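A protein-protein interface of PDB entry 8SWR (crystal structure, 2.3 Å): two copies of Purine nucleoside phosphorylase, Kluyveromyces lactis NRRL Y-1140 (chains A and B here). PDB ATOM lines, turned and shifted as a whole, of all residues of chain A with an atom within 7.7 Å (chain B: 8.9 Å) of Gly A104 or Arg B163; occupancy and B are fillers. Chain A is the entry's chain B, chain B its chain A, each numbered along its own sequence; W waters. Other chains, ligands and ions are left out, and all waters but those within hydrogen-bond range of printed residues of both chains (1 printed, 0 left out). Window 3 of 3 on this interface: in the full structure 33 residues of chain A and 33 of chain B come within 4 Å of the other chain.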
ATOM      1  N   HIS A 100     -25.235  -2.671  21.345  1.00  0.00           N
ATOM      2  CA  HIS A 100     -25.338  -1.250  21.630  1.00  0.00           C
ATOM      3  C   HIS A 100     -24.497  -0.454  20.646  1.00  0.00           C
ATOM      4  O   HIS A 100     -23.408  -0.884  20.253  1.00  0.00           O
ATOM      5  CB  HIS A 100     -24.894  -0.947  23.060  1.00  0.00           C
ATOM      6  CG  HIS A 100     -25.735  -1.609  24.106  1.00  0.00           C
ATOM      7  ND1 HIS A 100     -25.498  -2.891  24.551  1.00  0.00           N
ATOM      8  CD2 HIS A 100     -26.813  -1.164  24.796  1.00  0.00           C
ATOM      9  CE1 HIS A 100     -26.392  -3.208  25.471  1.00  0.00           C
ATOM     10  NE2 HIS A 100     -27.202  -2.178  25.638  1.00  0.00           N
ATOM     11  N   SER A 101     -25.012   0.716  20.258  1.00  0.00           N
ATOM     12  CA  SER A 101     -24.276   1.579  19.342  1.00  0.00           C
ATOM     13  C   SER A 101     -22.967   2.050  19.959  1.00  0.00           C
ATOM     14  O   SER A 101     -21.957   2.186  19.258  1.00  0.00           O
ATOM     15  CB  SER A 101     -25.138   2.775  18.940  1.00  0.00           C
ATOM     16  OG  SER A 101     -24.489   3.559  17.954  1.00  0.00           O
ATOM     17  N   TYR A 102     -22.957   2.293  21.274  1.00  0.00           N
ATOM     18  CA  TYR A 102     -21.733   2.735  21.931  1.00  0.00           C
ATOM     19  C   TYR A 102     -20.630   1.687  21.878  1.00  0.00           C
ATOM     20  O   TYR A 102     -19.472   2.016  22.159  1.00  0.00           O
ATOM     21  CB  TYR A 102     -22.016   3.144  23.385  1.00  0.00           C
ATOM     22  CG  TYR A 102     -22.525   2.053  24.311  1.00  0.00           C
ATOM     23  CD1 TYR A 102     -21.703   1.004  24.713  1.00  0.00           C
ATOM     24  CD2 TYR A 102     -23.818   2.097  24.818  1.00  0.00           C
ATOM     25  CE1 TYR A 102     -22.163   0.018  25.567  1.00  0.00           C
ATOM     26  CE2 TYR A 102     -24.285   1.118  25.676  1.00  0.00           C
ATOM     27  CZ  TYR A 102     -23.456   0.080  26.046  1.00  0.00           C
ATOM     28  OH  TYR A 102     -23.925  -0.896  26.897  1.00  0.00           O
ATOM     29  N   GLU A 103     -20.957   0.443  21.531  1.00  0.00           N
ATOM     30  CA  GLU A 103     -19.959  -0.603  21.348  1.00  0.00           C
ATOM     31  C   GLU A 103     -19.265  -0.528  19.994  1.00  0.00           C
ATOM     32  O   GLU A 103     -18.417  -1.379  19.703  1.00  0.00           O
ATOM     33  CB  GLU A 103     -20.604  -1.984  21.519  1.00  0.00           C
ATOM     34  CG  GLU A 103     -20.543  -2.529  22.940  1.00  0.00           C
ATOM     35  CD  GLU A 103     -19.122  -2.771  23.422  1.00  0.00           C
ATOM     36  OE1 GLU A 103     -18.914  -2.822  24.653  1.00  0.00           O
ATOM     37  OE2 GLU A 103     -18.218  -2.924  22.573  1.00  0.00           O
ATOM     38  N   GLY A 104     -19.599   0.461  19.164  1.00  0.00           N
ATOM     39  CA  GLY A 104     -19.010   0.598  17.853  1.00  0.00           C
ATOM     40  C   GLY A 104     -19.813  -0.020  16.728  1.00  0.00           C
ATOM     41  O   GLY A 104     -19.511   0.246  15.557  1.00  0.00           O
ATOM     42  N   HIS A 105     -20.822  -0.827  17.045  1.00  0.00           N
ATOM     43  CA  HIS A 105     -21.620  -1.471  16.017  1.00  0.00           C
ATOM     44  C   HIS A 105     -22.494  -0.448  15.297  1.00  0.00           C
ATOM     45  O   HIS A 105     -22.822   0.619  15.826  1.00  0.00           O
ATOM     46  CB  HIS A 105     -22.493  -2.566  16.630  1.00  0.00           C
ATOM     47  CG  HIS A 105     -21.720  -3.633  17.339  1.00  0.00           C
ATOM     48  ND1 HIS A 105     -20.569  -4.185  16.823  1.00  0.00           N
ATOM     49  CD2 HIS A 105     -21.922  -4.230  18.537  1.00  0.00           C
ATOM     50  CE1 HIS A 105     -20.103  -5.091  17.665  1.00  0.00           C
ATOM     51  NE2 HIS A 105     -20.905  -5.137  18.714  1.00  0.00           N
ATOM     52  N   SER A 106     -22.864  -0.786  14.067  1.00  0.00           N
ATOM     53  CA  SER A 106     -23.772   0.047  13.298  1.00  0.00           C
ATOM     54  C   SER A 106     -25.213  -0.219  13.723  1.00  0.00           C
ATOM     55  O   SER A 106     -25.542  -1.276  14.270  1.00  0.00           O
ATOM     56  CB  SER A 106     -23.606  -0.206  11.799  1.00  0.00           C
ATOM     57  OG  SER A 106     -23.767  -1.580  11.492  1.00  0.00           O
ATOM     58  N   LEU A 107     -26.076   0.769  13.471  1.00  0.00           N
ATOM     59  CA  LEU A 107     -27.488   0.613  13.810  1.00  0.00           C
ATOM     60  C   LEU A 107     -28.100  -0.579  13.088  1.00  0.00           C
ATOM     61  O   LEU A 107     -29.033  -1.205  13.604  1.00  0.00           O
ATOM     62  CB  LEU A 107     -28.256   1.899  13.487  1.00  0.00           C
ATOM     63  CG  LEU A 107     -28.778   2.159  12.066  1.00  0.00           C
ATOM     64  CD1 LEU A 107     -30.185   1.594  11.848  1.00  0.00           C
ATOM     65  CD2 LEU A 107     -28.750   3.647  11.755  1.00  0.00           C
ATOM     66  N   GLU A 109     -26.561  -3.529  12.312  1.00  0.00           N
ATOM     67  CA  GLU A 109     -26.184  -4.751  13.016  1.00  0.00           C
ATOM     68  C   GLU A 109     -27.012  -4.941  14.280  1.00  0.00           C
ATOM     69  O   GLU A 109     -27.398  -6.069  14.614  1.00  0.00           O
ATOM     70  CB  GLU A 109     -24.693  -4.723  13.358  1.00  0.00           C
ATOM     71  CG  GLU A 109     -23.773  -5.115  12.212  1.00  0.00           C
ATOM     72  CD  GLU A 109     -22.332  -4.703  12.454  1.00  0.00           C
ATOM     73  OE1 GLU A 109     -21.951  -4.532  13.632  1.00  0.00           O
ATOM     74  OE2 GLU A 109     -21.582  -4.552  11.467  1.00  0.00           O
ATOM     75  N   THR A 110     -27.306  -3.848  14.990  1.00  0.00           N
ATOM     76  CA  THR A 110     -28.049  -3.936  16.243  1.00  0.00           C
ATOM     77  C   THR A 110     -29.506  -4.326  16.033  1.00  0.00           C
ATOM     78  O   THR A 110     -30.142  -4.821  16.970  1.00  0.00           O
ATOM     79  CB  THR A 110     -27.985  -2.602  16.991  1.00  0.00           C
ATOM     80  OG1 THR A 110     -28.232  -1.527  16.077  1.00  0.00           O
ATOM     81  CG2 THR A 110     -26.614  -2.406  17.618  1.00  0.00           C
ATOM     82  N   HIS A 211     -26.418   8.315  23.195  1.00  0.00           N
ATOM     83  CA  HIS A 211     -25.490   7.315  22.677  1.00  0.00           C
ATOM     84  C   HIS A 211     -24.704   6.632  23.790  1.00  0.00           C
ATOM     85  O   HIS A 211     -24.446   5.426  23.719  1.00  0.00           O
ATOM     86  CB  HIS A 211     -24.547   7.962  21.663  1.00  0.00           C
ATOM     87  CG  HIS A 211     -23.619   6.999  20.994  1.00  0.00           C
ATOM     88  ND1 HIS A 211     -22.382   6.678  21.511  1.00  0.00           N
ATOM     89  CD2 HIS A 211     -23.745   6.288  19.849  1.00  0.00           C
ATOM     90  CE1 HIS A 211     -21.785   5.816  20.709  1.00  0.00           C
ATOM     91  NE2 HIS A 211     -22.591   5.559  19.695  1.00  0.00           N
ATOM     92  N   GLY A 212     -24.313   7.378  24.821  1.00  0.00           N
ATOM     93  CA  GLY A 212     -23.428   6.851  25.832  1.00  0.00           C
ATOM     94  C   GLY A 212     -22.020   6.713  25.287  1.00  0.00           C
ATOM     95  O   GLY A 212     -21.692   7.266  24.234  1.00  0.00           O
ATOM     96  N   PRO A 213     -21.155   5.956  25.982  1.00  0.00           N
ATOM     97  CA  PRO A 213     -21.420   5.204  27.211  1.00  0.00           C
ATOM     98  C   PRO A 213     -21.169   6.005  28.488  1.00  0.00           C
ATOM     99  O   PRO A 213     -21.080   5.420  29.567  1.00  0.00           O
ATOM    100  CB  PRO A 213     -20.438   4.041  27.107  1.00  0.00           C
ATOM    101  CG  PRO A 213     -19.257   4.648  26.428  1.00  0.00           C
ATOM    102  CD  PRO A 213     -19.803   5.681  25.463  1.00  0.00           C
ATOM    103  N   ASP B   7     -10.931  -0.202  14.663  1.00  0.00           N
ATOM    104  CA  ASP B   7     -10.528  -1.437  15.326  1.00  0.00           C
ATOM    105  C   ASP B   7      -9.745  -1.120  16.595  1.00  0.00           C
ATOM    106  O   ASP B   7      -8.907  -0.219  16.610  1.00  0.00           O
ATOM    107  CB  ASP B   7      -9.697  -2.292  14.363  1.00  0.00           C
ATOM    108  CG  ASP B   7      -9.220  -3.602  14.974  1.00  0.00           C
ATOM    109  OD1 ASP B   7      -8.463  -4.308  14.279  1.00  0.00           O
ATOM    110  OD2 ASP B   7      -9.617  -3.954  16.110  1.00  0.00           O
ATOM    111  N   ILE B   8     -10.015  -1.886  17.649  1.00  0.00           N
ATOM    112  CA  ILE B   8      -9.384  -1.629  18.940  1.00  0.00           C
ATOM    113  C   ILE B   8      -7.993  -2.246  19.001  1.00  0.00           C
ATOM    114  O   ILE B   8      -7.059  -1.640  19.538  1.00  0.00           O
ATOM    115  CB  ILE B   8     -10.288  -2.132  20.082  1.00  0.00           C
ATOM    116  CG1 ILE B   8      -9.594  -1.953  21.432  1.00  0.00           C
ATOM    117  CG2 ILE B   8     -10.695  -3.584  19.859  1.00  0.00           C
ATOM    118  CD1 ILE B   8     -10.525  -1.538  22.546  1.00  0.00           C
ATOM    119  N   GLN B  11      -5.840  -0.106  17.355  1.00  0.00           N
ATOM    120  CA  GLN B  11      -5.681   1.092  18.171  1.00  0.00           C
ATOM    121  C   GLN B  11      -4.714   0.844  19.319  1.00  0.00           C
ATOM    122  O   GLN B  11      -3.929   1.728  19.680  1.00  0.00           O
ATOM    123  CB  GLN B  11      -7.041   1.543  18.698  1.00  0.00           C
ATOM    124  CG  GLN B  11      -7.746   2.567  17.823  1.00  0.00           C
ATOM    125  CD  GLN B  11      -8.705   3.441  18.609  1.00  0.00           C
ATOM    126  OE1 GLN B  11      -9.894   3.139  18.703  1.00  0.00           O
ATOM    127  NE2 GLN B  11      -8.193   4.529  19.174  1.00  0.00           N
ATOM    128  N   LEU B 107     -12.531  11.342  16.458  1.00  0.00           N
ATOM    129  CA  LEU B 107     -12.342  11.684  17.863  1.00  0.00           C
ATOM    130  C   LEU B 107     -11.302  10.781  18.511  1.00  0.00           C
ATOM    131  O   LEU B 107     -10.537  11.219  19.378  1.00  0.00           O
ATOM    132  CB  LEU B 107     -13.676  11.594  18.604  1.00  0.00           C
ATOM    133  CG  LEU B 107     -14.702  12.657  18.210  1.00  0.00           C
ATOM    134  CD1 LEU B 107     -16.025  12.415  18.908  1.00  0.00           C
ATOM    135  CD2 LEU B 107     -14.174  14.045  18.536  1.00  0.00           C
ATOM    136  N   ALA B 108     -11.251   9.515  18.089  1.00  0.00           N
ATOM    137  CA  ALA B 108     -10.237   8.602  18.600  1.00  0.00           C
ATOM    138  C   ALA B 108      -8.836   9.068  18.225  1.00  0.00           C
ATOM    139  O   ALA B 108      -7.891   8.905  19.004  1.00  0.00           O
ATOM    140  CB  ALA B 108     -10.492   7.188  18.079  1.00  0.00           C
ATOM    141  N   VAL B 111      -7.801  12.175  20.442  1.00  0.00           N
ATOM    142  CA  VAL B 111      -7.499  11.854  21.832  1.00  0.00           C
ATOM    143  C   VAL B 111      -6.542  10.685  21.966  1.00  0.00           C
ATOM    144  O   VAL B 111      -6.232  10.281  23.097  1.00  0.00           O
ATOM    145  CB  VAL B 111      -8.783  11.587  22.641  1.00  0.00           C
ATOM    146  CG1 VAL B 111      -9.792  12.702  22.418  1.00  0.00           C
ATOM    147  CG2 VAL B 111      -9.372  10.236  22.266  1.00  0.00           C
ATOM    148  N   ARG B 115      -4.066   8.695  25.446  1.00  0.00           N
ATOM    149  CA  ARG B 115      -3.925   7.279  25.765  1.00  0.00           C
ATOM    150  C   ARG B 115      -2.462   6.858  25.789  1.00  0.00           C
ATOM    151  O   ARG B 115      -2.023   6.148  26.701  1.00  0.00           O
ATOM    152  CB  ARG B 115      -4.706   6.439  24.755  1.00  0.00           C
ATOM    153  CG  ARG B 115      -6.177   6.783  24.668  1.00  0.00           C
ATOM    154  CD  ARG B 115      -6.999   5.690  25.307  1.00  0.00           C
ATOM    155  NE  ARG B 115      -8.432   5.870  25.119  1.00  0.00           N
ATOM    156  CZ  ARG B 115      -9.332   5.704  26.078  1.00  0.00           C
ATOM    157  NH1 ARG B 115      -8.975   5.387  27.312  1.00  0.00           N
ATOM    158  NH2 ARG B 115     -10.622   5.856  25.790  1.00  0.00           N
ATOM    159  N   PRO B 154     -22.725  16.633  20.910  1.00  0.00           N
ATOM    160  CA  PRO B 154     -22.382  15.624  19.891  1.00  0.00           C
ATOM    161  C   PRO B 154     -22.239  14.225  20.460  1.00  0.00           C
ATOM    162  O   PRO B 154     -22.574  13.250  19.778  1.00  0.00           O
ATOM    163  CB  PRO B 154     -21.054  16.134  19.311  1.00  0.00           C
ATOM    164  CG  PRO B 154     -20.963  17.554  19.689  1.00  0.00           C
ATOM    165  CD  PRO B 154     -21.726  17.714  20.965  1.00  0.00           C
ATOM    166  N   GLY B 155     -21.747  14.098  21.695  1.00  0.00           N
ATOM    167  CA  GLY B 155     -21.675  12.789  22.317  1.00  0.00           C
ATOM    168  C   GLY B 155     -23.044  12.181  22.555  1.00  0.00           C
ATOM    169  O   GLY B 155     -23.243  10.979  22.364  1.00  0.00           O
ATOM    170  N   CYS B 157     -25.439  12.545  20.670  1.00  0.00           N
ATOM    171  CA  CYS B 157     -25.966  12.237  19.349  1.00  0.00           C
ATOM    172  C   CYS B 157     -25.062  11.301  18.552  1.00  0.00           C
ATOM    173  O   CYS B 157     -25.229  11.177  17.334  1.00  0.00           O
ATOM    174  CB  CYS B 157     -26.216  13.529  18.569  1.00  0.00           C
ATOM    175  SG  CYS B 157     -27.431  14.636  19.335  1.00  0.00           S
ATOM    176  N   GLY B 158     -24.104  10.649  19.206  1.00  0.00           N
ATOM    177  CA  GLY B 158     -23.357   9.564  18.602  1.00  0.00           C
ATOM    178  C   GLY B 158     -21.917   9.870  18.250  1.00  0.00           C
ATOM    179  O   GLY B 158     -21.199   8.955  17.826  1.00  0.00           O
ATOM    180  N   PHE B 159     -21.467  11.114  18.398  1.00  0.00           N
ATOM    181  CA  PHE B 159     -20.085  11.486  18.094  1.00  0.00           C
ATOM    182  C   PHE B 159     -19.351  11.593  19.428  1.00  0.00           C
ATOM    183  O   PHE B 159     -19.273  12.662  20.039  1.00  0.00           O
ATOM    184  CB  PHE B 159     -20.029  12.771  17.274  1.00  0.00           C
ATOM    185  CG  PHE B 159     -20.740  12.668  15.944  1.00  0.00           C
ATOM    186  CD1 PHE B 159     -22.118  12.805  15.870  1.00  0.00           C
ATOM    187  CD2 PHE B 159     -20.035  12.415  14.775  1.00  0.00           C
ATOM    188  CE1 PHE B 159     -22.780  12.703  14.658  1.00  0.00           C
ATOM    189  CE2 PHE B 159     -20.697  12.311  13.555  1.00  0.00           C
ATOM    190  CZ  PHE B 159     -22.069  12.456  13.500  1.00  0.00           C
ATOM    191  N   HIS B 160     -18.796  10.463  19.869  1.00  0.00           N
ATOM    192  CA  HIS B 160     -18.301  10.298  21.220  1.00  0.00           C
ATOM    193  C   HIS B 160     -16.905   9.683  21.217  1.00  0.00           C
ATOM    194  O   HIS B 160     -16.661   8.709  20.480  1.00  0.00           O
ATOM    195  CB  HIS B 160     -19.283   9.412  21.992  1.00  0.00           C
ATOM    196  CG  HIS B 160     -19.167   9.516  23.478  1.00  0.00           C
ATOM    197  ND1 HIS B 160     -18.081   9.029  24.171  1.00  0.00           N
ATOM    198  CD2 HIS B 160     -20.002  10.039  24.405  1.00  0.00           C
ATOM    199  CE1 HIS B 160     -18.249   9.254  25.461  1.00  0.00           C
ATOM    200  NE2 HIS B 160     -19.406   9.866  25.631  1.00  0.00           N
ATOM    201  N   PRO B 161     -15.976  10.210  22.023  1.00  0.00           N
ATOM    202  CA  PRO B 161     -14.608   9.661  22.024  1.00  0.00           C
ATOM    203  C   PRO B 161     -14.512   8.244  22.562  1.00  0.00           C
ATOM    204  O   PRO B 161     -13.532   7.551  22.257  1.00  0.00           O
ATOM    205  CB  PRO B 161     -13.829  10.640  22.914  1.00  0.00           C
ATOM    206  CG  PRO B 161     -14.864  11.326  23.738  1.00  0.00           C
ATOM    207  CD  PRO B 161     -16.121  11.366  22.924  1.00  0.00           C
ATOM    208  N   LEU B 162     -15.479   7.788  23.355  1.00  0.00           N
ATOM    209  CA  LEU B 162     -15.441   6.445  23.912  1.00  0.00           C
ATOM    210  C   LEU B 162     -16.224   5.433  23.086  1.00  0.00           C
ATOM    211  O   LEU B 162     -16.298   4.264  23.478  1.00  0.00           O
ATOM    212  CB  LEU B 162     -15.970   6.453  25.349  1.00  0.00           C
ATOM    213  CG  LEU B 162     -15.227   7.366  26.325  1.00  0.00           C
ATOM    214  CD1 LEU B 162     -15.742   7.183  27.745  1.00  0.00           C
ATOM    215  CD2 LEU B 162     -13.733   7.102  26.252  1.00  0.00           C
ATOM    216  N   ARG B 163     -16.808   5.850  21.962  1.00  0.00           N
ATOM    217  CA  ARG B 163     -17.525   4.922  21.099  1.00  0.00           C
ATOM    218  C   ARG B 163     -16.590   3.823  20.613  1.00  0.00           C
ATOM    219  O   ARG B 163     -15.424   4.070  20.294  1.00  0.00           O
ATOM    220  CB  ARG B 163     -18.135   5.661  19.905  1.00  0.00           C
ATOM    221  CG  ARG B 163     -18.801   4.750  18.886  1.00  0.00           C
ATOM    222  CD  ARG B 163     -19.721   5.514  17.949  1.00  0.00           C
ATOM    223  NE  ARG B 163     -20.774   4.654  17.422  1.00  0.00           N
ATOM    224  CZ  ARG B 163     -20.793   4.162  16.190  1.00  0.00           C
ATOM    225  NH1 ARG B 163     -19.834   4.439  15.321  1.00  0.00           N
ATOM    226  NH2 ARG B 163     -21.799   3.374  15.822  1.00  0.00           N
ATOM    227  N   GLY B 164     -17.105   2.600  20.564  1.00  0.00           N
ATOM    228  CA  GLY B 164     -16.298   1.448  20.225  1.00  0.00           C
ATOM    229  C   GLY B 164     -15.974   0.614  21.448  1.00  0.00           C
ATOM    230  O   GLY B 164     -16.314   0.949  22.586  1.00  0.00           O
ATOM    231  N   ALA B 165     -15.302  -0.506  21.184  1.00  0.00           N
ATOM    232  CA  ALA B 165     -14.921  -1.427  22.244  1.00  0.00           C
ATOM    233  C   ALA B 165     -14.135  -0.702  23.328  1.00  0.00           C
ATOM    234  O   ALA B 165     -13.298   0.157  23.042  1.00  0.00           O
ATOM    235  CB  ALA B 165     -14.093  -2.580  21.672  1.00  0.00           C
ATOM    236  N   ASN B 166     -14.421  -1.048  24.579  1.00  0.00           N
ATOM    237  CA  ASN B 166     -13.822  -0.342  25.701  1.00  0.00           C
ATOM    238  C   ASN B 166     -12.363  -0.737  25.883  1.00  0.00           C
ATOM    239  O   ASN B 166     -11.997  -1.909  25.760  1.00  0.00           O
ATOM    240  CB  ASN B 166     -14.601  -0.628  26.984  1.00  0.00           C
ATOM    241  CG  ASN B 166     -14.120   0.205  28.154  1.00  0.00           C
ATOM    242  OD1 ASN B 166     -14.234   1.431  28.146  1.00  0.00           O
ATOM    243  ND2 ASN B 166     -13.574  -0.458  29.166  1.00  0.00           N
ATOM    244  N   PHE B 167     -11.526   0.259  26.176  1.00  0.00           N
ATOM    245  CA  PHE B 167     -10.133   0.030  26.555  1.00  0.00           C
ATOM    246  C   PHE B 167     -10.119  -0.385  28.025  1.00  0.00           C
ATOM    247  O   PHE B 167      -9.868   0.413  28.931  1.00  0.00           O
ATOM    248  CB  PHE B 167      -9.295   1.282  26.320  1.00  0.00           C
ATOM    249  CG  PHE B 167      -9.033   1.580  24.873  1.00  0.00           C
ATOM    250  CD1 PHE B 167      -8.002   0.947  24.195  1.00  0.00           C
ATOM    251  CD2 PHE B 167      -9.807   2.505  24.193  1.00  0.00           C
ATOM    252  CE1 PHE B 167      -7.757   1.226  22.863  1.00  0.00           C
ATOM    253  CE2 PHE B 167      -9.567   2.789  22.861  1.00  0.00           C
ATOM    254  CZ  PHE B 167      -8.540   2.148  22.196  1.00  0.00           C
ATOM    255  N   ARG B 173     -16.275   0.660  31.275  1.00  0.00           N
ATOM    256  CA  ARG B 173     -17.121   0.756  30.091  1.00  0.00           C
ATOM    257  C   ARG B 173     -18.067   1.946  30.192  1.00  0.00           C
ATOM    258  O   ARG B 173     -18.291   2.660  29.207  1.00  0.00           O
ATOM    259  CB  ARG B 173     -17.906  -0.543  29.901  1.00  0.00           C
ATOM    260  CG  ARG B 173     -19.084  -0.439  28.942  1.00  0.00           C
ATOM    261  CD  ARG B 173     -18.641  -0.561  27.496  1.00  0.00           C
ATOM    262  NE  ARG B 173     -18.089   0.688  26.985  1.00  0.00           N
ATOM    263  CZ  ARG B 173     -17.764   0.894  25.716  1.00  0.00           C
ATOM    264  NH1 ARG B 173     -17.933  -0.043  24.800  1.00  0.00           N
ATOM    265  NH2 ARG B 173     -17.256   2.072  25.360  1.00  0.00           N
ATOM    266  N   VAL B 241     -13.081  13.931  28.595  1.00  0.00           N
ATOM    267  CA  VAL B 241     -13.708  12.621  28.773  1.00  0.00           C
ATOM    268  C   VAL B 241     -12.653  11.522  28.736  1.00  0.00           C
ATOM    269  O   VAL B 241     -12.645  10.615  29.576  1.00  0.00           O
ATOM    270  CB  VAL B 241     -14.797  12.398  27.705  1.00  0.00           C
ATOM    271  CG1 VAL B 241     -15.288  10.959  27.730  1.00  0.00           C
ATOM    272  CG2 VAL B 241     -15.954  13.360  27.917  1.00  0.00           C
ATOM    273  N   THR B 242     -11.736  11.599  27.769  1.00  0.00           N
ATOM    274  CA  THR B 242     -10.692  10.585  27.656  1.00  0.00           C
ATOM    275  C   THR B 242      -9.752  10.620  28.855  1.00  0.00           C
ATOM    276  O   THR B 242      -9.317   9.569  29.339  1.00  0.00           O
ATOM    277  CB  THR B 242      -9.916  10.779  26.352  1.00  0.00           C
ATOM    278  OG1 THR B 242     -10.829  10.775  25.248  1.00  0.00           O
ATOM    279  CG2 THR B 242      -8.899   9.663  26.160  1.00  0.00           C
ATOM    280  N   HIS B 245     -11.571   8.968  31.712  1.00  0.00           N
ATOM    281  CA  HIS B 245     -11.576   7.521  31.518  1.00  0.00           C
ATOM    282  C   HIS B 245     -10.261   6.894  31.969  1.00  0.00           C
ATOM    283  O   HIS B 245     -10.244   5.775  32.494  1.00  0.00           O
ATOM    284  CB  HIS B 245     -11.849   7.195  30.050  1.00  0.00           C
ATOM    285  CG  HIS B 245     -12.102   5.742  29.795  1.00  0.00           C
ATOM    286  ND1 HIS B 245     -11.147   4.904  29.261  1.00  0.00           N
ATOM    287  CD2 HIS B 245     -13.200   4.978  30.000  1.00  0.00           C
ATOM    288  CE1 HIS B 245     -11.645   3.686  29.148  1.00  0.00           C
ATOM    289  NE2 HIS B 245     -12.890   3.704  29.590  1.00  0.00           N
HETATM  290  O   HOH W   1     -24.271  10.188  25.532  1.00  0.00           O
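Water W1 lies within hydrogen-bond range of N of Gly A212 (2.9 Å) and O of Gly B155 (3.4 Å).
Among the printed residues, merely in contact across the chains: Gly A212 with His B160 (3.3 Å), Pro A213 with Arg B173 (3.3 Å), His A211 with Gly B155 (3.4 Å), His A211 with Gly B158 (3.5 Å), Glu A103 with Ala B165 (3.6 Å), Glu A103 with Gly B164 (3.6 Å), Gly A104 with Gly B164 (3.6 Å), Tyr A102 with Arg B163 (3.7 Å), Tyr A102 with Arg B173 (3.7 Å), Gly A104 with Arg B163 (3.9 Å), Pro A213 with His B160 (3.9 Å) and Pro A213 with Leu B162 (3.9 Å).
Printed residues of chain B within 4 Å of Glu A103: Gly B164, Ala B165 and Arg B173.
Gly A104 touches just these residues of chain B: Arg B163 (3.9 Å) and Gly B164 (3.6 Å).
Of the printed residues of chain B, His A211 touches Gly B155, Gly B158 and Arg B163.
Of the printed residues of chain A, His B160 touches Gly A212 and Pro A213.
Pro B161 touches none of the printed residues of chain A.
Of the printed residues of chain A, Leu B162 touches Pro A213 (3.9 Å).
Of chain A, only Ser A101 (3.3 Å), Tyr A102 (3.7 Å), Gly A104 (3.9 Å), His A105 (2.9 Å) and His A211 (3.0 Å) come within 4 Å of Arg B163.
Of chain A, only Tyr A102 (2.9 Å), Glu A103 (3.6 Å) and Gly A104 (3.6 Å) come within 4 Å of Gly B164.
The nearest printed residue of chain A that does not touch Arg B163 is Pro A213 (4.6 Å).
Of the 24 printed residues of chain B, 8 touch a printed residue of chain A.
Of the 13 printed residues of chain A, 8 touch a printed residue of chain B.
The backbone carbonyl oxygen of Leu B162 sits at hydrogen-bond distance from the guanidinium group of Arg B173.
O of Gly B164 lies within hydrogen-bond range of NH1 of Arg B173 (2.9 Å).
The side-chain hydroxyl of Ser A101 lies within hydrogen-bond range of a ring nitrogen (NE2) of His A211, 3.3 Å away.
A ring nitrogen (ND1) of His A105 is in hydrogen-bond range of the side-chain carboxylate of Glu A109.
The side-chain hydroxyl (OH) of Tyr A102 lies close to a ring nitrogen (ND1) of His A100 (3.5 Å).
N of Leu B162 sits at hydrogen-bond distance from ND1 of His B160 (3.0 Å).
NE of Arg B163 sits at hydrogen-bond distance from O of Ser A101, at 3.3 Å.
The guanidinium group of Arg B173 lies within salt-bridge range of the side-chain carboxylate of Glu A103 (3.0 Å).
The backbone carbonyl oxygen of Tyr A102 lies within hydrogen-bond range of the backbone NH of Gly B164 (2.9 Å).
A ring nitrogen (NE2) of His A211 sits at hydrogen-bond distance from the guanidinium group of Arg B163, 3.0 Å away.
NH2 of Arg B163 lies within hydrogen-bond range of O of His A105 (2.9 Å).
1 position is printed for both chains.
Of the 17 pairs that touch across the chains among the printed residues, none has its exchanged pair printed and touching as well.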
